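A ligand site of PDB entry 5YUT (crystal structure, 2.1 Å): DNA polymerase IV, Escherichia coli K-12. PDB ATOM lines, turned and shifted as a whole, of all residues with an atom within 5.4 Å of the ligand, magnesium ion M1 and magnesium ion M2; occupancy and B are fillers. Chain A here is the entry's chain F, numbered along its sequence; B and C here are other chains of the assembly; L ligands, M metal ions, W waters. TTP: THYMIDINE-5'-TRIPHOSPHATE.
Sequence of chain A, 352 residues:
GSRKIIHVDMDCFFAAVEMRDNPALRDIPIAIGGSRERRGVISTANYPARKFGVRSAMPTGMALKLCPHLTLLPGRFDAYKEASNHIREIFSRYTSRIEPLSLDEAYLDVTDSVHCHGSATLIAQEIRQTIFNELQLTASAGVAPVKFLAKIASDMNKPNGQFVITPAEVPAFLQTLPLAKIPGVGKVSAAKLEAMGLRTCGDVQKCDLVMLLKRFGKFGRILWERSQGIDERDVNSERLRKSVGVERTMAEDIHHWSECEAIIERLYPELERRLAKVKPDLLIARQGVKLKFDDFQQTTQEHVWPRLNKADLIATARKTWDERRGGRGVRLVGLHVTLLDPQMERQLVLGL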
ATOM      1  N   ASP A   9      12.466  18.157  11.836  1.00  0.00           N
ATOM      2  CA  ASP A   9      12.672  17.593  10.504  1.00  0.00           C
ATOM      3  C   ASP A   9      12.138  18.584   9.480  1.00  0.00           C
ATOM      4  O   ASP A   9      10.934  18.849   9.463  1.00  0.00           O
ATOM      5  CB  ASP A   9      11.953  16.231  10.369  1.00  0.00           C
ATOM      6  CG  ASP A   9      12.369  15.455   9.119  1.00  0.00           C
ATOM      7  OD1 ASP A   9      12.567  16.093   8.079  1.00  0.00           O
ATOM      8  OD2 ASP A   9      12.496  14.209   9.182  1.00  0.00           O
ATOM      9  N   MET A  10      13.016  19.108   8.619  1.00  0.00           N
ATOM     10  CA  MET A  10      12.582  20.060   7.586  1.00  0.00           C
ATOM     11  C   MET A  10      11.701  19.367   6.554  1.00  0.00           C
ATOM     12  O   MET A  10      11.918  18.187   6.216  1.00  0.00           O
ATOM     13  CB  MET A  10      13.790  20.697   6.887  1.00  0.00           C
ATOM     14  CG  MET A  10      14.762  21.393   7.819  1.00  0.00           C
ATOM     15  SD  MET A  10      14.045  22.784   8.717  1.00  0.00           S
ATOM     16  CE  MET A  10      13.719  23.913   7.354  1.00  0.00           C
ATOM     17  N   ASP A  11      10.693  20.099   6.066  1.00  0.00           N
ATOM     18  CA  ASP A  11       9.741  19.567   5.078  1.00  0.00           C
ATOM     19  C   ASP A  11      10.333  19.653   3.675  1.00  0.00           C
ATOM     20  O   ASP A  11      10.747  20.732   3.223  1.00  0.00           O
ATOM     21  CB  ASP A  11       8.420  20.342   5.129  1.00  0.00           C
ATOM     22  CG  ASP A  11       7.757  20.346   6.518  1.00  0.00           C
ATOM     23  OD1 ASP A  11       7.649  19.285   7.160  1.00  0.00           O
ATOM     24  OD2 ASP A  11       7.309  21.416   6.971  1.00  0.00           O
ATOM     25  N   CYS A  12      10.342  18.517   2.962  1.00  0.00           N
ATOM     26  CA  CYS A  12      10.809  18.439   1.567  1.00  0.00           C
ATOM     27  C   CYS A  12      12.058  19.290   1.361  1.00  0.00           C
ATOM     28  O   CYS A  12      12.115  20.166   0.495  1.00  0.00           O
ATOM     29  CB  CYS A  12       9.704  18.857   0.589  1.00  0.00           C
ATOM     30  SG  CYS A  12       8.204  17.917   0.802  1.00  0.00           S
ATOM     31  N   PHE A  13      13.074  18.999   2.187  1.00  0.00           N
ATOM     32  CA  PHE A  13      14.125  19.970   2.467  1.00  0.00           C
ATOM     33  C   PHE A  13      14.741  20.558   1.188  1.00  0.00           C
ATOM     34  O   PHE A  13      14.636  21.776   0.963  1.00  0.00           O
ATOM     35  CB  PHE A  13      15.201  19.350   3.357  1.00  0.00           C
ATOM     36  CG  PHE A  13      16.305  20.317   3.711  1.00  0.00           C
ATOM     37  CD1 PHE A  13      16.004  21.610   4.098  1.00  0.00           C
ATOM     38  CD2 PHE A  13      17.634  19.931   3.620  1.00  0.00           C
ATOM     39  CE1 PHE A  13      17.016  22.514   4.424  1.00  0.00           C
ATOM     40  CE2 PHE A  13      18.658  20.821   3.947  1.00  0.00           C
ATOM     41  CZ  PHE A  13      18.363  22.113   4.340  1.00  0.00           C
ATOM     42  N   PHE A  14      15.395  19.736   0.355  1.00  0.00           N
ATOM     43  CA  PHE A  14      16.064  20.292  -0.824  1.00  0.00           C
ATOM     44  C   PHE A  14      15.064  21.053  -1.686  1.00  0.00           C
ATOM     45  O   PHE A  14      15.312  22.192  -2.099  1.00  0.00           O
ATOM     46  CB  PHE A  14      16.746  19.227  -1.694  1.00  0.00           C
ATOM     47  CG  PHE A  14      17.916  18.556  -1.061  1.00  0.00           C
ATOM     48  CD1 PHE A  14      18.321  18.867   0.222  1.00  0.00           C
ATOM     49  CD2 PHE A  14      18.620  17.580  -1.779  1.00  0.00           C
ATOM     50  CE1 PHE A  14      19.405  18.211   0.802  1.00  0.00           C
ATOM     51  CE2 PHE A  14      19.713  16.931  -1.208  1.00  0.00           C
ATOM     52  CZ  PHE A  14      20.096  17.239   0.084  1.00  0.00           C
ATOM     53  N   ALA A  15      13.904  20.437  -1.944  1.00  0.00           N
ATOM     54  CA  ALA A  15      12.871  21.068  -2.760  1.00  0.00           C
ATOM     55  C   ALA A  15      12.326  22.347  -2.111  1.00  0.00           C
ATOM     56  O   ALA A  15      12.044  23.327  -2.801  1.00  0.00           O
ATOM     57  CB  ALA A  15      11.734  20.078  -3.038  1.00  0.00           C
ATOM     58  N   ILE A  42      15.672  10.109  -7.659  1.00  0.00           N
ATOM     59  CA  ILE A  42      15.136  11.312  -7.016  1.00  0.00           C
ATOM     60  C   ILE A  42      15.757  11.433  -5.640  1.00  0.00           C
ATOM     61  O   ILE A  42      15.732  10.472  -4.865  1.00  0.00           O
ATOM     62  CB  ILE A  42      13.605  11.222  -6.910  1.00  0.00           C
ATOM     63  CG1 ILE A  42      12.978  11.080  -8.297  1.00  0.00           C
ATOM     64  CG2 ILE A  42      13.075  12.428  -6.153  1.00  0.00           C
ATOM     65  CD1 ILE A  42      13.315  12.210  -9.207  1.00  0.00           C
ATOM     66  N   SER A  43      16.316  12.612  -5.329  1.00  0.00           N
ATOM     67  CA  SER A  43      16.743  12.857  -3.961  1.00  0.00           C
ATOM     68  C   SER A  43      15.535  13.225  -3.098  1.00  0.00           C
ATOM     69  O   SER A  43      15.351  12.685  -1.999  1.00  0.00           O
ATOM     70  CB  SER A  43      17.795  13.972  -3.913  1.00  0.00           C
ATOM     71  OG  SER A  43      19.104  13.433  -4.020  1.00  0.00           O
ATOM     72  N   THR A  44      14.730  14.164  -3.582  1.00  0.00           N
ATOM     73  CA  THR A  44      13.453  14.476  -2.950  1.00  0.00           C
ATOM     74  C   THR A  44      12.593  15.233  -3.951  1.00  0.00           C
ATOM     75  O   THR A  44      13.072  15.638  -5.005  1.00  0.00           O
ATOM     76  CB  THR A  44      13.632  15.277  -1.660  1.00  0.00           C
ATOM     77  OG1 THR A  44      12.387  15.288  -0.958  1.00  0.00           O
ATOM     78  CG2 THR A  44      14.014  16.701  -1.951  1.00  0.00           C
ATOM     79  N   ALA A  45      11.325  15.399  -3.601  1.00  0.00           N
ATOM     80  CA  ALA A  45      10.341  16.032  -4.457  1.00  0.00           C
ATOM     81  C   ALA A  45       9.451  16.929  -3.609  1.00  0.00           C
ATOM     82  O   ALA A  45       9.336  16.763  -2.396  1.00  0.00           O
ATOM     83  CB  ALA A  45       9.494  14.985  -5.191  1.00  0.00           C
ATOM     84  N   TYR A  47       5.519  18.681  -2.875  1.00  0.00           N
ATOM     85  CA  TYR A  47       4.220  18.009  -2.751  1.00  0.00           C
ATOM     86  C   TYR A  47       3.458  17.902  -4.076  1.00  0.00           C
ATOM     87  O   TYR A  47       2.809  16.870  -4.327  1.00  0.00           O
ATOM     88  CB  TYR A  47       3.375  18.687  -1.673  1.00  0.00           C
ATOM     89  CG  TYR A  47       3.718  18.131  -0.288  1.00  0.00           C
ATOM     90  CD1 TYR A  47       3.208  16.916   0.130  1.00  0.00           C
ATOM     91  CD2 TYR A  47       4.604  18.788   0.569  1.00  0.00           C
ATOM     92  CE1 TYR A  47       3.542  16.374   1.378  1.00  0.00           C
ATOM     93  CE2 TYR A  47       4.935  18.259   1.823  1.00  0.00           C
ATOM     94  CZ  TYR A  47       4.397  17.057   2.213  1.00  0.00           C
ATOM     95  OH  TYR A  47       4.681  16.495   3.439  1.00  0.00           O
ATOM     96  N   ARG A  50       4.981  14.732  -5.417  1.00  0.00           N
ATOM     97  CA  ARG A  50       4.582  13.622  -4.555  1.00  0.00           C
ATOM     98  C   ARG A  50       3.152  13.171  -4.820  1.00  0.00           C
ATOM     99  O   ARG A  50       2.854  11.972  -4.704  1.00  0.00           O
ATOM    100  CB  ARG A  50       4.736  14.006  -3.077  1.00  0.00           C
ATOM    101  CG  ARG A  50       6.164  14.103  -2.655  1.00  0.00           C
ATOM    102  CD  ARG A  50       6.385  14.549  -1.211  1.00  0.00           C
ATOM    103  NE  ARG A  50       7.829  14.571  -0.996  1.00  0.00           N
ATOM    104  CZ  ARG A  50       8.442  14.717   0.171  1.00  0.00           C
ATOM    105  NH1 ARG A  50       7.736  14.873   1.288  1.00  0.00           N
ATOM    106  NH2 ARG A  50       9.769  14.714   0.198  1.00  0.00           N
ATOM    107  N   SER A  56      11.488   9.963  -2.823  1.00  0.00           N
ATOM    108  CA  SER A  56      12.937   9.798  -2.671  1.00  0.00           C
ATOM    109  C   SER A  56      13.351   8.369  -2.992  1.00  0.00           C
ATOM    110  O   SER A  56      12.627   7.412  -2.704  1.00  0.00           O
ATOM    111  CB  SER A  56      13.381  10.120  -1.235  1.00  0.00           C
ATOM    112  OG  SER A  56      13.128  11.467  -0.893  1.00  0.00           O
ATOM    113  N   ALA A  57      14.537   8.232  -3.589  1.00  0.00           N
ATOM    114  CA  ALA A  57      15.152   6.953  -3.957  1.00  0.00           C
ATOM    115  C   ALA A  57      14.492   6.313  -5.161  1.00  0.00           C
ATOM    116  O   ALA A  57      14.916   5.233  -5.589  1.00  0.00           O
ATOM    117  CB  ALA A  57      15.174   5.950  -2.795  1.00  0.00           C
ATOM    118  N   SER A 102      21.478  14.642   9.994  1.00  0.00           N
ATOM    119  CA  SER A 102      21.696  14.919   8.582  1.00  0.00           C
ATOM    120  C   SER A 102      21.607  16.425   8.428  1.00  0.00           C
ATOM    121  O   SER A 102      21.448  17.129   9.433  1.00  0.00           O
ATOM    122  CB  SER A 102      20.652  14.219   7.712  1.00  0.00           C
ATOM    123  OG  SER A 102      19.330  14.619   8.066  1.00  0.00           O
ATOM    124  N   ASP A 104      19.127  18.174   7.495  1.00  0.00           N
ATOM    125  CA  ASP A 104      17.819  18.782   7.715  1.00  0.00           C
ATOM    126  C   ASP A 104      17.124  18.355   9.016  1.00  0.00           C
ATOM    127  O   ASP A 104      15.946  18.691   9.188  1.00  0.00           O
ATOM    128  CB  ASP A 104      16.918  18.497   6.500  1.00  0.00           C
ATOM    129  CG  ASP A 104      16.109  17.219   6.655  1.00  0.00           C
ATOM    130  OD1 ASP A 104      16.581  16.226   7.240  1.00  0.00           O
ATOM    131  OD2 ASP A 104      14.951  17.239   6.164  1.00  0.00           O
ATOM    132  N   GLU A 105      17.805  17.653   9.923  1.00  0.00           N
ATOM    133  CA  GLU A 105      17.107  17.156  11.096  1.00  0.00           C
ATOM    134  C   GLU A 105      18.043  16.979  12.279  1.00  0.00           C
ATOM    135  O   GLU A 105      19.256  16.823  12.125  1.00  0.00           O
ATOM    136  CB  GLU A 105      16.326  15.859  10.787  1.00  0.00           C
ATOM    137  CG  GLU A 105      17.136  14.574  10.606  1.00  0.00           C
ATOM    138  CD  GLU A 105      16.268  13.338  10.267  1.00  0.00           C
ATOM    139  OE1 GLU A 105      15.600  13.326   9.209  1.00  0.00           O
ATOM    140  OE2 GLU A 105      16.257  12.373  11.041  1.00  0.00           O
ATOM    141  N   ASP A 155       6.876  12.663  11.733  1.00  0.00           N
ATOM    142  CA  ASP A 155       6.326  12.335  10.427  1.00  0.00           C
ATOM    143  C   ASP A 155       4.818  12.435  10.373  1.00  0.00           C
ATOM    144  O   ASP A 155       4.256  12.440   9.263  1.00  0.00           O
ATOM    145  CB  ASP A 155       6.709  10.913  10.021  1.00  0.00           C
ATOM    146  CG  ASP A 155       7.996  10.844   9.280  1.00  0.00           C
ATOM    147  OD1 ASP A 155       8.547  11.925   8.947  1.00  0.00           O
ATOM    148  OD2 ASP A 155       8.458   9.717   9.040  1.00  0.00           O
ATOM    149  N   LYS A 158       3.282  16.089   9.321  1.00  0.00           N
ATOM    150  CA  LYS A 158       3.980  16.718   8.196  1.00  0.00           C
ATOM    151  C   LYS A 158       2.994  17.053   7.076  1.00  0.00           C
ATOM    152  O   LYS A 158       2.105  16.271   6.813  1.00  0.00           O
ATOM    153  CB  LYS A 158       5.056  15.790   7.631  1.00  0.00           C
ATOM    154  CG  LYS A 158       6.402  15.965   8.228  1.00  0.00           C
ATOM    155  CD  LYS A 158       7.443  15.056   7.585  1.00  0.00           C
ATOM    156  CE  LYS A 158       8.851  15.420   8.083  1.00  0.00           C
ATOM    157  NZ  LYS A 158       9.283  16.808   7.628  1.00  0.00           N
ATOM    158  P    DC B  18      15.580   8.374   7.722  1.00  0.00           P
ATOM    159  OP1  DC B  18      14.674   9.007   8.668  1.00  0.00           O
ATOM    160  OP2  DC B  18      15.001   7.588   6.602  1.00  0.00           O
ATOM    161  O5'  DC B  18      16.498   9.513   7.012  1.00  0.00           O
ATOM    162  C5'  DC B  18      17.441  10.281   7.795  1.00  0.00           C
ATOM    163  C4'  DC B  18      18.200  11.237   6.890  1.00  0.00           C
ATOM    164  O4'  DC B  18      19.166  10.506   6.103  1.00  0.00           O
ATOM    165  C3'  DC B  18      17.317  11.991   5.899  1.00  0.00           C
ATOM    166  O3'  DC B  18      17.030  13.243   6.397  1.00  0.00           O
ATOM    167  C2'  DC B  18      18.161  12.093   4.641  1.00  0.00           C
ATOM    168  C1'  DC B  18      19.220  11.028   4.786  1.00  0.00           C
ATOM    169  N1   DC B  18      19.127   9.905   3.814  1.00  0.00           N
ATOM    170  C2   DC B  18      19.858   9.986   2.646  1.00  0.00           C
ATOM    171  O2   DC B  18      20.525  11.019   2.416  1.00  0.00           O
ATOM    172  N3   DC B  18      19.842   8.940   1.780  1.00  0.00           N
ATOM    173  C4   DC B  18      19.111   7.855   2.042  1.00  0.00           C
ATOM    174  N4   DC B  18      19.138   6.866   1.138  1.00  0.00           N
ATOM    175  C5   DC B  18      18.329   7.749   3.231  1.00  0.00           C
ATOM    176  C6   DC B  18      18.376   8.796   4.094  1.00  0.00           C
ATOM    177  P    DA C   4      21.507   4.037  -8.730  1.00  0.00           P
ATOM    178  OP1  DA C   4      22.398   3.525  -9.803  1.00  0.00           O
ATOM    179  OP2  DA C   4      21.543   3.331  -7.433  1.00  0.00           O
ATOM    180  O5'  DA C   4      21.753   5.573  -8.397  1.00  0.00           O
ATOM    181  C5'  DA C   4      21.770   6.536  -9.399  1.00  0.00           C
ATOM    182  C4'  DA C   4      22.513   7.775  -8.909  1.00  0.00           C
ATOM    183  O4'  DA C   4      21.789   8.411  -7.820  1.00  0.00           O
ATOM    184  C3'  DA C   4      23.916   7.518  -8.379  1.00  0.00           C
ATOM    185  O3'  DA C   4      24.756   8.633  -8.666  1.00  0.00           O
ATOM    186  C2'  DA C   4      23.697   7.360  -6.859  1.00  0.00           C
ATOM    187  C1'  DA C   4      22.507   8.286  -6.600  1.00  0.00           C
ATOM    188  N9   DA C   4      21.582   7.761  -5.613  1.00  0.00           N
ATOM    189  C8   DA C   4      21.194   6.468  -5.444  1.00  0.00           C
ATOM    190  N7   DA C   4      20.321   6.302  -4.477  1.00  0.00           N
ATOM    191  C5   DA C   4      20.127   7.570  -3.987  1.00  0.00           C
ATOM    192  C6   DA C   4      19.313   8.068  -2.939  1.00  0.00           C
ATOM    193  N6   DA C   4      18.517   7.298  -2.190  1.00  0.00           N
ATOM    194  N1   DA C   4      19.344   9.396  -2.716  1.00  0.00           N
ATOM    195  C2   DA C   4      20.152  10.161  -3.480  1.00  0.00           C
ATOM    196  N3   DA C   4      20.953   9.798  -4.479  1.00  0.00           N
ATOM    197  C4   DA C   4      20.889   8.482  -4.680  1.00  0.00           C
ATOM    198  P    DG C   5      26.311   8.584  -8.300  1.00  0.00           P
ATOM    199  OP1  DG C   5      26.961   9.449  -9.321  1.00  0.00           O
ATOM    200  OP2  DG C   5      26.730   7.153  -8.107  1.00  0.00           O
ATOM    201  O5'  DG C   5      26.394   9.281  -6.890  1.00  0.00           O
ATOM    202  C5'  DG C   5      26.108  10.646  -6.777  1.00  0.00           C
ATOM    203  C4'  DG C   5      26.322  11.069  -5.358  1.00  0.00           C
ATOM    204  O4'  DG C   5      25.223  10.601  -4.517  1.00  0.00           O
ATOM    205  C3'  DG C   5      27.600  10.503  -4.739  1.00  0.00           C
ATOM    206  O3'  DG C   5      28.151  11.502  -3.942  1.00  0.00           O
ATOM    207  C2'  DG C   5      27.098   9.337  -3.877  1.00  0.00           C
ATOM    208  C1'  DG C   5      25.753   9.883  -3.418  1.00  0.00           C
ATOM    209  N9   DG C   5      24.805   8.861  -2.970  1.00  0.00           N
ATOM    210  C8   DG C   5      24.747   7.538  -3.357  1.00  0.00           C
ATOM    211  N7   DG C   5      23.797   6.870  -2.766  1.00  0.00           N
ATOM    212  C5   DG C   5      23.174   7.809  -1.935  1.00  0.00           C
ATOM    213  C6   DG C   5      22.073   7.673  -1.040  1.00  0.00           C
ATOM    214  O6   DG C   5      21.377   6.669  -0.805  1.00  0.00           O
ATOM    215  N1   DG C   5      21.777   8.874  -0.406  1.00  0.00           N
ATOM    216  C2   DG C   5      22.451  10.036  -0.595  1.00  0.00           C
ATOM    217  N2   DG C   5      22.009  11.088   0.117  1.00  0.00           N
ATOM    218  N3   DG C   5      23.478  10.182  -1.407  1.00  0.00           N
ATOM    219  C4   DG C   5      23.779   9.031  -2.054  1.00  0.00           C
HETATM  220  PA  TTP L   1      14.237  13.601   4.468  1.00  0.00           P
HETATM  221  O1A TTP L   1      13.836  14.438   5.667  1.00  0.00           O
HETATM  222  O2A TTP L   1      14.142  12.110   4.676  1.00  0.00           O
HETATM  223  O3A TTP L   1      13.181  13.904   3.286  1.00  0.00           O
HETATM  224  PB  TTP L   1      12.537  15.336   2.967  1.00  0.00           P
HETATM  225  O1B TTP L   1      12.838  15.733   1.527  1.00  0.00           O
HETATM  226  O2B TTP L   1      12.965  16.463   3.857  1.00  0.00           O
HETATM  227  O3B TTP L   1      10.983  14.969   3.072  1.00  0.00           O
HETATM  228  PG  TTP L   1      10.084  15.164   4.405  1.00  0.00           P
HETATM  229  O1G TTP L   1      10.925  15.162   5.688  1.00  0.00           O
HETATM  230  O2G TTP L   1       9.187  13.944   4.352  1.00  0.00           O
HETATM  231  O3G TTP L   1       9.287  16.441   4.258  1.00  0.00           O
HETATM  232  O5' TTP L   1      15.657  13.980   3.828  1.00  0.00           O
HETATM  233  C5' TTP L   1      16.179  15.314   3.830  1.00  0.00           C
HETATM  234  C4' TTP L   1      16.890  15.533   2.482  1.00  0.00           C
HETATM  235  O4' TTP L   1      17.836  14.480   2.277  1.00  0.00           O
HETATM  236  C3' TTP L   1      15.930  15.434   1.299  1.00  0.00           C
HETATM  237  O3' TTP L   1      15.215  16.651   1.025  1.00  0.00           O
HETATM  238  C2' TTP L   1      16.858  14.988   0.165  1.00  0.00           C
HETATM  239  C1' TTP L   1      17.909  14.140   0.871  1.00  0.00           C
HETATM  240  N1  TTP L   1      17.603  12.712   0.679  1.00  0.00           N
HETATM  241  C2  TTP L   1      18.242  12.030  -0.370  1.00  0.00           C
HETATM  242  O2  TTP L   1      19.072  12.651  -1.075  1.00  0.00           O
HETATM  243  N3  TTP L   1      18.004  10.725  -0.603  1.00  0.00           N
HETATM  244  C4  TTP L   1      17.110  10.052   0.135  1.00  0.00           C
HETATM  245  O4  TTP L   1      16.864   8.846  -0.073  1.00  0.00           O
HETATM  246  C5  TTP L   1      16.393  10.739   1.225  1.00  0.00           C
HETATM  247  C5M TTP L   1      15.393   9.960   2.047  1.00  0.00           C
HETATM  248  C6  TTP L   1      16.680  12.092   1.441  1.00  0.00           C
HETATM  249 MG    MG M   1      12.924  16.180   6.086  1.00  0.00          MG
HETATM  250 MG    MG M   2      15.310  14.297   7.606  1.00  0.00          MG
HETATM  251  O   HOH W   1       9.420  11.637   2.850  1.00  0.00           O
HETATM  252  O   HOH W   2      13.472  12.311   7.913  1.00  0.00           O
HETATM  253  O   HOH W   3      11.422  11.999   1.100  1.00  0.00           O
HETATM  254  O   HOH W   4      11.189  12.776   7.049  1.00  0.00           O
HETATM  255  O   HOH W   5       6.914  17.536   4.596  1.00  0.00           O
HETATM  256  O   HOH W   6      15.661   6.591   0.927  1.00  0.00           O
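The backbone NH of Phe 14 is in hydrogen-bond range of an oxygen (O3') of the ligand (3.2 Å).
The backbone NH (N) of Phe 13 lies within hydrogen-bond range of an oxygen (O1B) of the ligand, at 3.3 Å.
The side-chain hydroxyl of Thr 44 lies within hydrogen-bond range of an oxygen (O1B) of the ligand, 2.6 Å away.
A nitrogen (N3) of the ligand lies within hydrogen-bond range of N1 of DA 4 of chain C (2.8 Å).
N3 of DC 18 of chain B sits close to a nitrogen (N3) of the ligand (3.5 Å).
The guanidinium group of Arg 50 lies within salt-bridge range of an oxygen (O1B) of the ligand.
An oxygen (O3G) of the ligand is in hydrogen-bond range of the backbone NH (N) of Cys 12 (2.7 Å).
An oxygen (O3G) of the ligand lies within salt-bridge range of the side-chain amino group of Lys 158.
OG of Ser 43 is in hydrogen-bond range of O2 of the ligand (3.0 Å).
The side-chain sulfur (SG) of Cys 12 sits at hydrogen-bond distance from the backbone carbonyl oxygen (O) of Ala 45 (3.6 Å).
O of Asp 9 lies within hydrogen-bond range of NZ of Lys 158 (3.2 Å).
The side-chain hydroxyl (OG) of Ser 56 lies within hydrogen-bond range of the backbone carbonyl oxygen (O) of Ser 43, at 2.8 Å.
NE of Arg 50 sits at hydrogen-bond distance from O of Ala 45 (3.0 Å).
The side-chain carboxylate (OD1) of Asp 11 lies within salt-bridge range of the side-chain amino group (NZ) of Lys 158, at 3.0 Å.
The backbone carbonyl oxygen (O) of Met 10 sits close to the side-chain amino group (NZ) of Lys 158, at 3.3 Å.
N2 of DG 5 of chain C sits close to O2 of DC 18 of chain B (2.7 Å).
OD1 of Asp 104 sits close to OG of Ser 102.
Asp 11 touches the ligand.
Ser 56 touches the ligand (CB to C5M, 3.9 Å).
N2 of DG 5 of chain C touches O2 of the ligand, at 3.5 Å.
Hydrophobic or aromatic side chains within 4 Å of the ligand: Phe 13 and Phe 14.
Of the 23 residues printed, 15 come within 4 Å of the ligand.
Of the 23 residues printed, 3 come within 4 Å of magnesium ion M1.
Along chain A the residues within 4 Å of magnesium ion M1 span positions 9 to 104.
Magnesium ion M1 is bound by O1A of the ligand (2.0 Å), OD1 of Asp 9 (2.0 Å), O2B of the ligand (2.2 Å), O of Met 10 (2.2 Å), O1G of the ligand (2.3 Å) and OD2 of Asp 104 (2.3 Å).
Magnesium ion M1 has six donor atoms within binding distance.
Magnesium ion M2 is bound by OE1 of Glu 105, at 1.9 Å.
Magnesium ion M2 is bound by OD1 of Asp 104, at 2.3 Å.
O3' of DC 18 of chain B binds magnesium ion M2, 2.4 Å away.
Magnesium ion M2 is bound by O1A of the ligand.
Slightly farther from magnesium ion M2 lies water W2 (2.7 Å).
Water W2 lies within hydrogen-bond range of OD2 of Asp 9 (2.5 Å) and O2A of the ligand (3.3 Å).
Water W5 lies within hydrogen-bond range of an oxygen (O3G) of the ligand (2.6 Å), the side-chain hydroxyl of Tyr 47 (2.7 Å) and the side-chain carboxylate of Asp 11 (3.2 Å).
Water W6 lies within hydrogen-bond range of an oxygen (O4) of the ligand (2.7 Å) and N4 of DC 18 of chain B (3.5 Å).
Water W4 lies within hydrogen-bond range of the side-chain carboxylate (OD2) of Asp 9 and the side-chain carboxylate (OD1) of Asp 155.
Water W3 lies within hydrogen-bond range of OG of Ser 56, NH2 of Arg 50 and O3A of the ligand.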
